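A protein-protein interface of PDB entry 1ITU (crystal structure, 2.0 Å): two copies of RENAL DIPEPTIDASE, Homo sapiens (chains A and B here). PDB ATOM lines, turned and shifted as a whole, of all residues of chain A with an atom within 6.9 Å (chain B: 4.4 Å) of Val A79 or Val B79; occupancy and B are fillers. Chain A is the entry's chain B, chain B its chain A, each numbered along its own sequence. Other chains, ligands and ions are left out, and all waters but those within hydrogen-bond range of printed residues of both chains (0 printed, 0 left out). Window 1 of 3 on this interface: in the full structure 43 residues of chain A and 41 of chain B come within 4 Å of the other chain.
Val A79 touches Val B79 (CG1 to CG1, 3.99 Å).
Val A79 touches Leu B83 (CG1 to CD1, 3.9 Å).
O of Arg A80 touches CG2 of Val B136, 3.7 Å away.
CD1 of Leu A83 touches CG1 of Val B79, at 3.6 Å.
Leu A83 touches Val B136 (CD1 to CG1, 3.8 Å).
O of Arg B80 touches CG2 of Val A136, at 3.7 Å.
CG1 of Val A136 touches CD1 of Leu B83, 3.8 Å away.
The side-chain carboxylate of Asp B131 lies within salt-bridge range of the guanidinium group of Arg A80.
NE of Arg B80 lies within salt-bridge range of OD1 of Asp A131 (3.2 Å).
Along chain A the printed residues that touch a printed residue of chain B span positions 79 to 136.
Val A79 touches Leu B83, and with the chains exchanged Leu A83 touches Val B79.
Arg A80 touches Asp B131, and with the chains exchanged Asp A131 touches Arg B80.
Arg A80 touches Val B136, and with the chains exchanged Val A136 touches Arg B80.
Leu A83 touches Val B136, and with the chains exchanged Val A136 touches Leu B83.
10 positions are printed for both chains.
Of the 9 pairs that touch across the chains among the printed residues, 9 have their exchanged pair printed and touching as well.
Of the printed residues of chain B, Val A79 touches Val B79 (3.99 Å) and Leu B83 (3.9 Å).
Thr A82 touches none of the printed residues of chain B.
Of the printed residues of chain B, Leu A83 touches Val B79 and Val B136.
Of the printed residues of chain B, Val A136 touches Arg B80 (3.7 Å) and Leu B83 (3.8 Å).
Of the printed residues of chain A, Val B79 touches Val A79 and Leu A83.
Ser B129 touches none of the printed residues of chain A.
The nearest printed residue of chain B that does not touch Val A79 is Arg B80 (4.3 Å).
NH2 of Arg A80 is in salt-bridge range of OE2 of Glu A84, 3.4 Å away.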
ATOM      1  N   THR A  69      22.970  16.921   6.092  1.00  0.00           N
ATOM      2  CA  THR A  69      21.616  16.770   6.593  1.00  0.00           C
ATOM      3  C   THR A  69      21.058  15.622   5.739  1.00  0.00           C
ATOM      4  O   THR A  69      21.257  15.596   4.521  1.00  0.00           O
ATOM      5  CB  THR A  69      20.801  18.089   6.445  1.00  0.00           C
ATOM      6  OG1 THR A  69      19.493  17.888   6.981  1.00  0.00           O
ATOM      7  CG2 THR A  69      20.692  18.529   4.996  1.00  0.00           C
ATOM      8  N   THR A  73      15.311  15.049   4.916  1.00  0.00           N
ATOM      9  CA  THR A  73      15.099  16.417   5.377  1.00  0.00           C
ATOM     10  C   THR A  73      14.770  17.277   4.158  1.00  0.00           C
ATOM     11  O   THR A  73      14.311  18.412   4.306  1.00  0.00           O
ATOM     12  CB  THR A  73      16.306  17.009   6.126  1.00  0.00           C
ATOM     13  OG1 THR A  73      17.421  17.130   5.237  1.00  0.00           O
ATOM     14  CG2 THR A  73      16.679  16.154   7.318  1.00  0.00           C
ATOM     15  N   LYS A  76      11.671  19.463   3.718  1.00  0.00           N
ATOM     16  CA  LYS A  76      11.280  19.543   5.117  1.00  0.00           C
ATOM     17  C   LYS A  76      12.145  20.600   5.811  1.00  0.00           C
ATOM     18  O   LYS A  76      12.003  21.795   5.533  1.00  0.00           O
ATOM     19  CB  LYS A  76      11.397  18.182   5.801  1.00  0.00           C
ATOM     20  CG  LYS A  76      10.255  17.250   5.441  1.00  0.00           C
ATOM     21  CD  LYS A  76      10.196  16.082   6.378  1.00  0.00           C
ATOM     22  CE  LYS A  76       8.940  15.270   6.144  1.00  0.00           C
ATOM     23  NZ  LYS A  76       8.802  14.232   7.209  1.00  0.00           N
ATOM     24  N   ASP A  77      13.069  20.171   6.667  1.00  0.00           N
ATOM     25  CA  ASP A  77      13.940  21.117   7.374  1.00  0.00           C
ATOM     26  C   ASP A  77      15.423  21.090   6.967  1.00  0.00           C
ATOM     27  O   ASP A  77      16.295  21.447   7.756  1.00  0.00           O
ATOM     28  CB  ASP A  77      13.800  20.934   8.892  1.00  0.00           C
ATOM     29  CG  ASP A  77      14.102  19.518   9.350  1.00  0.00           C
ATOM     30  OD1 ASP A  77      14.222  19.333  10.571  1.00  0.00           O
ATOM     31  OD2 ASP A  77      14.208  18.585   8.516  1.00  0.00           O
ATOM     32  N   ALA A  78      15.693  20.730   5.712  1.00  0.00           N
ATOM     33  CA  ALA A  78      17.061  20.656   5.190  1.00  0.00           C
ATOM     34  C   ALA A  78      17.858  21.951   5.326  1.00  0.00           C
ATOM     35  O   ALA A  78      19.037  21.919   5.677  1.00  0.00           O
ATOM     36  CB  ALA A  78      17.051  20.190   3.711  1.00  0.00           C
ATOM     37  N   VAL A  79      17.232  23.082   4.999  1.00  0.00           N
ATOM     38  CA  VAL A  79      17.909  24.366   5.092  1.00  0.00           C
ATOM     39  C   VAL A  79      18.217  24.716   6.551  1.00  0.00           C
ATOM     40  O   VAL A  79      19.342  25.086   6.875  1.00  0.00           O
ATOM     41  CB  VAL A  79      17.110  25.482   4.400  1.00  0.00           C
ATOM     42  CG1 VAL A  79      17.904  26.786   4.412  1.00  0.00           C
ATOM     43  CG2 VAL A  79      16.780  25.072   2.971  1.00  0.00           C
ATOM     44  N   ARG A  80      17.243  24.529   7.438  1.00  0.00           N
ATOM     45  CA  ARG A  80      17.441  24.792   8.871  1.00  0.00           C
ATOM     46  C   ARG A  80      18.617  23.974   9.418  1.00  0.00           C
ATOM     47  O   ARG A  80      19.538  24.514  10.018  1.00  0.00           O
ATOM     48  CB  ARG A  80      16.181  24.409   9.648  1.00  0.00           C
ATOM     49  CG  ARG A  80      16.248  24.651  11.158  1.00  0.00           C
ATOM     50  CD  ARG A  80      15.105  23.903  11.824  1.00  0.00           C
ATOM     51  NE  ARG A  80      14.866  24.298  13.209  1.00  0.00           N
ATOM     52  CZ  ARG A  80      15.236  23.581  14.267  1.00  0.00           C
ATOM     53  NH1 ARG A  80      14.966  24.017  15.500  1.00  0.00           N
ATOM     54  NH2 ARG A  80      15.899  22.435  14.096  1.00  0.00           N
ATOM     55  N   ARG A  81      18.589  22.668   9.185  1.00  0.00           N
ATOM     56  CA  ARG A  81      19.651  21.794   9.672  1.00  0.00           C
ATOM     57  C   ARG A  81      21.021  22.026   9.043  1.00  0.00           C
ATOM     58  O   ARG A  81      22.037  21.801   9.692  1.00  0.00           O
ATOM     59  CB  ARG A  81      19.237  20.327   9.578  1.00  0.00           C
ATOM     60  CG  ARG A  81      18.045  20.016  10.460  1.00  0.00           C
ATOM     61  CD  ARG A  81      17.884  18.514  10.680  1.00  0.00           C
ATOM     62  NE  ARG A  81      16.882  18.231  11.705  1.00  0.00           N
ATOM     63  CZ  ARG A  81      17.098  18.348  13.013  1.00  0.00           C
ATOM     64  NH1 ARG A  81      16.127  18.078  13.873  1.00  0.00           N
ATOM     65  NH2 ARG A  81      18.290  18.723  13.464  1.00  0.00           N
ATOM     66  N   THR A  82      21.055  22.482   7.793  1.00  0.00           N
ATOM     67  CA  THR A  82      22.331  22.780   7.143  1.00  0.00           C
ATOM     68  C   THR A  82      22.981  23.972   7.849  1.00  0.00           C
ATOM     69  O   THR A  82      24.190  23.984   8.088  1.00  0.00           O
ATOM     70  CB  THR A  82      22.138  23.100   5.652  1.00  0.00           C
ATOM     71  OG1 THR A  82      21.587  21.945   4.996  1.00  0.00           O
ATOM     72  CG2 THR A  82      23.465  23.473   5.007  1.00  0.00           C
ATOM     73  N   LEU A  83      22.157  24.957   8.216  1.00  0.00           N
ATOM     74  CA  LEU A  83      22.633  26.142   8.936  1.00  0.00           C
ATOM     75  C   LEU A  83      23.161  25.738  10.309  1.00  0.00           C
ATOM     76  O   LEU A  83      24.222  26.185  10.726  1.00  0.00           O
ATOM     77  CB  LEU A  83      21.508  27.180   9.077  1.00  0.00           C
ATOM     78  CG  LEU A  83      21.031  27.772   7.751  1.00  0.00           C
ATOM     79  CD1 LEU A  83      20.031  28.906   7.985  1.00  0.00           C
ATOM     80  CD2 LEU A  83      22.210  28.287   6.976  1.00  0.00           C
ATOM     81  N   GLU A  84      22.429  24.877  11.008  1.00  0.00           N
ATOM     82  CA  GLU A  84      22.859  24.404  12.317  1.00  0.00           C
ATOM     83  C   GLU A  84      24.158  23.615  12.223  1.00  0.00           C
ATOM     84  O   GLU A  84      24.990  23.686  13.124  1.00  0.00           O
ATOM     85  CB  GLU A  84      21.796  23.520  12.941  1.00  0.00           C
ATOM     86  CG  GLU A  84      20.486  24.217  13.171  1.00  0.00           C
ATOM     87  CD  GLU A  84      19.525  23.344  13.928  1.00  0.00           C
ATOM     88  OE1 GLU A  84      19.406  22.144  13.596  1.00  0.00           O
ATOM     89  OE2 GLU A  84      18.899  23.848  14.877  1.00  0.00           O
ATOM     90  N   HIS A 128      20.217  19.189  -1.757  1.00  0.00           N
ATOM     91  CA  HIS A 128      18.935  19.416  -1.079  1.00  0.00           C
ATOM     92  C   HIS A 128      19.085  20.426   0.074  1.00  0.00           C
ATOM     93  O   HIS A 128      18.091  20.831   0.678  1.00  0.00           O
ATOM     94  CB  HIS A 128      18.302  18.101  -0.579  1.00  0.00           C
ATOM     95  CG  HIS A 128      19.154  17.336   0.386  1.00  0.00           C
ATOM     96  ND1 HIS A 128      20.305  16.680   0.004  1.00  0.00           N
ATOM     97  CD2 HIS A 128      19.021  17.121   1.717  1.00  0.00           C
ATOM     98  CE1 HIS A 128      20.846  16.097   1.058  1.00  0.00           C
ATOM     99  NE2 HIS A 128      20.087  16.349   2.109  1.00  0.00           N
ATOM    100  N   SER A 129      20.329  20.815   0.361  1.00  0.00           N
ATOM    101  CA  SER A 129      20.643  21.801   1.392  1.00  0.00           C
ATOM    102  C   SER A 129      20.327  23.220   0.935  1.00  0.00           C
ATOM    103  O   SER A 129      20.155  24.107   1.771  1.00  0.00           O
ATOM    104  CB  SER A 129      22.111  21.717   1.800  1.00  0.00           C
ATOM    105  OG  SER A 129      22.324  20.601   2.646  1.00  0.00           O
ATOM    106  N   ILE A 130      20.279  23.448  -0.382  1.00  0.00           N
ATOM    107  CA  ILE A 130      19.953  24.781  -0.902  1.00  0.00           C
ATOM    108  C   ILE A 130      18.480  24.898  -1.283  1.00  0.00           C
ATOM    109  O   ILE A 130      18.008  25.979  -1.631  1.00  0.00           O
ATOM    110  CB  ILE A 130      20.812  25.195  -2.133  1.00  0.00           C
ATOM    111  CG1 ILE A 130      20.476  24.335  -3.353  1.00  0.00           C
ATOM    112  CG2 ILE A 130      22.279  25.109  -1.811  1.00  0.00           C
ATOM    113  CD1 ILE A 130      21.059  24.877  -4.625  1.00  0.00           C
ATOM    114  N   ASP A 131      17.764  23.781  -1.216  1.00  0.00           N
ATOM    115  CA  ASP A 131      16.346  23.714  -1.559  1.00  0.00           C
ATOM    116  C   ASP A 131      16.023  24.433  -2.880  1.00  0.00           C
ATOM    117  O   ASP A 131      15.128  25.283  -2.946  1.00  0.00           O
ATOM    118  CB  ASP A 131      15.483  24.249  -0.404  1.00  0.00           C
ATOM    119  CG  ASP A 131      14.031  23.796  -0.492  1.00  0.00           C
ATOM    120  OD1 ASP A 131      13.153  24.509   0.030  1.00  0.00           O
ATOM    121  OD2 ASP A 131      13.756  22.727  -1.078  1.00  0.00           O
ATOM    122  N   VAL A 136      19.732  30.821  -1.498  1.00  0.00           N
ATOM    123  CA  VAL A 136      20.196  29.989  -0.386  1.00  0.00           C
ATOM    124  C   VAL A 136      21.633  29.525  -0.664  1.00  0.00           C
ATOM    125  O   VAL A 136      22.452  29.442   0.252  1.00  0.00           O
ATOM    126  CB  VAL A 136      19.288  28.765  -0.164  1.00  0.00           C
ATOM    127  CG1 VAL A 136      19.910  27.815   0.877  1.00  0.00           C
ATOM    128  CG2 VAL A 136      17.918  29.218   0.308  1.00  0.00           C
ATOM    129  N   LEU A 140      24.847  30.138   1.717  1.00  0.00           N
ATOM    130  CA  LEU A 140      25.719  29.077   2.227  1.00  0.00           C
ATOM    131  C   LEU A 140      27.161  29.421   1.885  1.00  0.00           C
ATOM    132  O   LEU A 140      28.060  29.159   2.672  1.00  0.00           O
ATOM    133  CB  LEU A 140      25.316  27.701   1.674  1.00  0.00           C
ATOM    134  CG  LEU A 140      23.907  27.197   2.005  1.00  0.00           C
ATOM    135  CD1 LEU A 140      23.761  25.739   1.617  1.00  0.00           C
ATOM    136  CD2 LEU A 140      23.636  27.341   3.490  1.00  0.00           C
ATOM    137  N   ASP B  77       8.629  26.909   4.629  1.00  0.00           N
ATOM    138  CA  ASP B  77       9.886  27.368   4.034  1.00  0.00           C
ATOM    139  C   ASP B  77      10.393  28.732   4.550  1.00  0.00           C
ATOM    140  O   ASP B  77      11.103  29.443   3.845  1.00  0.00           O
ATOM    141  CB  ASP B  77       9.773  27.377   2.501  1.00  0.00           C
ATOM    142  CG  ASP B  77       8.612  28.244   1.984  1.00  0.00           C
ATOM    143  OD1 ASP B  77       8.546  28.452   0.757  1.00  0.00           O
ATOM    144  OD2 ASP B  77       7.764  28.719   2.779  1.00  0.00           O
ATOM    145  N   ALA B  78      10.067  29.076   5.794  1.00  0.00           N
ATOM    146  CA  ALA B  78      10.494  30.353   6.380  1.00  0.00           C
ATOM    147  C   ALA B  78      11.996  30.589   6.304  1.00  0.00           C
ATOM    148  O   ALA B  78      12.428  31.643   5.862  1.00  0.00           O
ATOM    149  CB  ALA B  78      10.015  30.474   7.853  1.00  0.00           C
ATOM    150  N   VAL B  79      12.796  29.607   6.720  1.00  0.00           N
ATOM    151  CA  VAL B  79      14.250  29.770   6.694  1.00  0.00           C
ATOM    152  C   VAL B  79      14.774  29.994   5.269  1.00  0.00           C
ATOM    153  O   VAL B  79      15.554  30.914   5.014  1.00  0.00           O
ATOM    154  CB  VAL B  79      14.987  28.577   7.360  1.00  0.00           C
ATOM    155  CG1 VAL B  79      16.465  28.884   7.481  1.00  0.00           C
ATOM    156  CG2 VAL B  79      14.391  28.278   8.740  1.00  0.00           C
ATOM    157  N   ARG B  80      14.308  29.175   4.337  1.00  0.00           N
ATOM    158  CA  ARG B  80      14.728  29.298   2.952  1.00  0.00           C
ATOM    159  C   ARG B  80      14.455  30.706   2.429  1.00  0.00           C
ATOM    160  O   ARG B  80      15.357  31.367   1.924  1.00  0.00           O
ATOM    161  CB  ARG B  80      13.973  28.285   2.097  1.00  0.00           C
ATOM    162  CG  ARG B  80      14.230  28.391   0.599  1.00  0.00           C
ATOM    163  CD  ARG B  80      13.134  27.653  -0.149  1.00  0.00           C
ATOM    164  NE  ARG B  80      13.512  27.320  -1.520  1.00  0.00           N
ATOM    165  CZ  ARG B  80      13.087  27.968  -2.601  1.00  0.00           C
ATOM    166  NH1 ARG B  80      13.493  27.576  -3.805  1.00  0.00           N
ATOM    167  NH2 ARG B  80      12.281  29.018  -2.481  1.00  0.00           N
ATOM    168  N   ARG B  81      13.211  31.166   2.560  1.00  0.00           N
ATOM    169  CA  ARG B  81      12.846  32.496   2.072  1.00  0.00           C
ATOM    170  C   ARG B  81      13.546  33.641   2.779  1.00  0.00           C
ATOM    171  O   ARG B  81      13.818  34.663   2.158  1.00  0.00           O
ATOM    172  CB  ARG B  81      11.335  32.679   2.070  1.00  0.00           C
ATOM    173  CG  ARG B  81      10.645  31.709   1.122  1.00  0.00           C
ATOM    174  CD  ARG B  81       9.178  32.041   0.975  1.00  0.00           C
ATOM    175  NE  ARG B  81       8.570  31.350  -0.155  1.00  0.00           N
ATOM    176  CZ  ARG B  81       8.796  31.662  -1.425  1.00  0.00           C
ATOM    177  NH1 ARG B  81       8.199  30.975  -2.387  1.00  0.00           N
ATOM    178  NH2 ARG B  81       9.621  32.654  -1.737  1.00  0.00           N
ATOM    179  N   THR B  82      13.877  33.453   4.060  1.00  0.00           N
ATOM    180  CA  THR B  82      14.596  34.473   4.822  1.00  0.00           C
ATOM    181  C   THR B  82      15.969  34.691   4.198  1.00  0.00           C
ATOM    182  O   THR B  82      16.376  35.830   3.992  1.00  0.00           O
ATOM    183  CB  THR B  82      14.764  34.071   6.302  1.00  0.00           C
ATOM    184  OG1 THR B  82      13.472  33.984   6.909  1.00  0.00           O
ATOM    185  CG2 THR B  82      15.587  35.102   7.058  1.00  0.00           C
ATOM    186  N   LEU B  83      16.654  33.594   3.848  1.00  0.00           N
ATOM    187  CA  LEU B  83      17.986  33.664   3.228  1.00  0.00           C
ATOM    188  C   LEU B  83      17.896  34.329   1.855  1.00  0.00           C
ATOM    189  O   LEU B  83      18.755  35.118   1.479  1.00  0.00           O
ATOM    190  CB  LEU B  83      18.615  32.266   3.085  1.00  0.00           C
ATOM    191  CG  LEU B  83      18.828  31.358   4.299  1.00  0.00           C
ATOM    192  CD1 LEU B  83      19.739  30.187   3.903  1.00  0.00           C
ATOM    193  CD2 LEU B  83      19.456  32.136   5.447  1.00  0.00           C
ATOM    194  N   SER B 129      11.493  33.086  11.324  1.00  0.00           N
ATOM    195  CA  SER B 129      12.611  33.015  10.395  1.00  0.00           C
ATOM    196  C   SER B 129      13.734  32.109  10.897  1.00  0.00           C
ATOM    197  O   SER B 129      14.533  31.625  10.106  1.00  0.00           O
ATOM    198  CB  SER B 129      13.170  34.412  10.129  1.00  0.00           C
ATOM    199  OG  SER B 129      12.351  35.117   9.212  1.00  0.00           O
ATOM    200  N   ASP B 131      13.084  29.407  12.819  1.00  0.00           N
ATOM    201  CA  ASP B 131      12.460  28.107  13.081  1.00  0.00           C
ATOM    202  C   ASP B 131      12.936  27.484  14.410  1.00  0.00           C
ATOM    203  O   ASP B 131      13.340  26.319  14.464  1.00  0.00           O
ATOM    204  CB  ASP B 131      12.677  27.139  11.908  1.00  0.00           C
ATOM    205  CG  ASP B 131      11.781  25.903  11.987  1.00  0.00           C
ATOM    206  OD1 ASP B 131      12.127  24.877  11.367  1.00  0.00           O
ATOM    207  OD2 ASP B 131      10.728  25.946  12.665  1.00  0.00           O
ATOM    208  N   VAL B 136      20.526  28.682  13.485  1.00  0.00           N
ATOM    209  CA  VAL B 136      20.010  29.476  12.367  1.00  0.00           C
ATOM    210  C   VAL B 136      20.118  30.961  12.757  1.00  0.00           C
ATOM    211  O   VAL B 136      20.497  31.801  11.944  1.00  0.00           O
ATOM    212  CB  VAL B 136      18.529  29.112  12.035  1.00  0.00           C
ATOM    213  CG1 VAL B 136      17.952  30.069  10.973  1.00  0.00           C
ATOM    214  CG2 VAL B 136      18.442  27.680  11.532  1.00  0.00           C
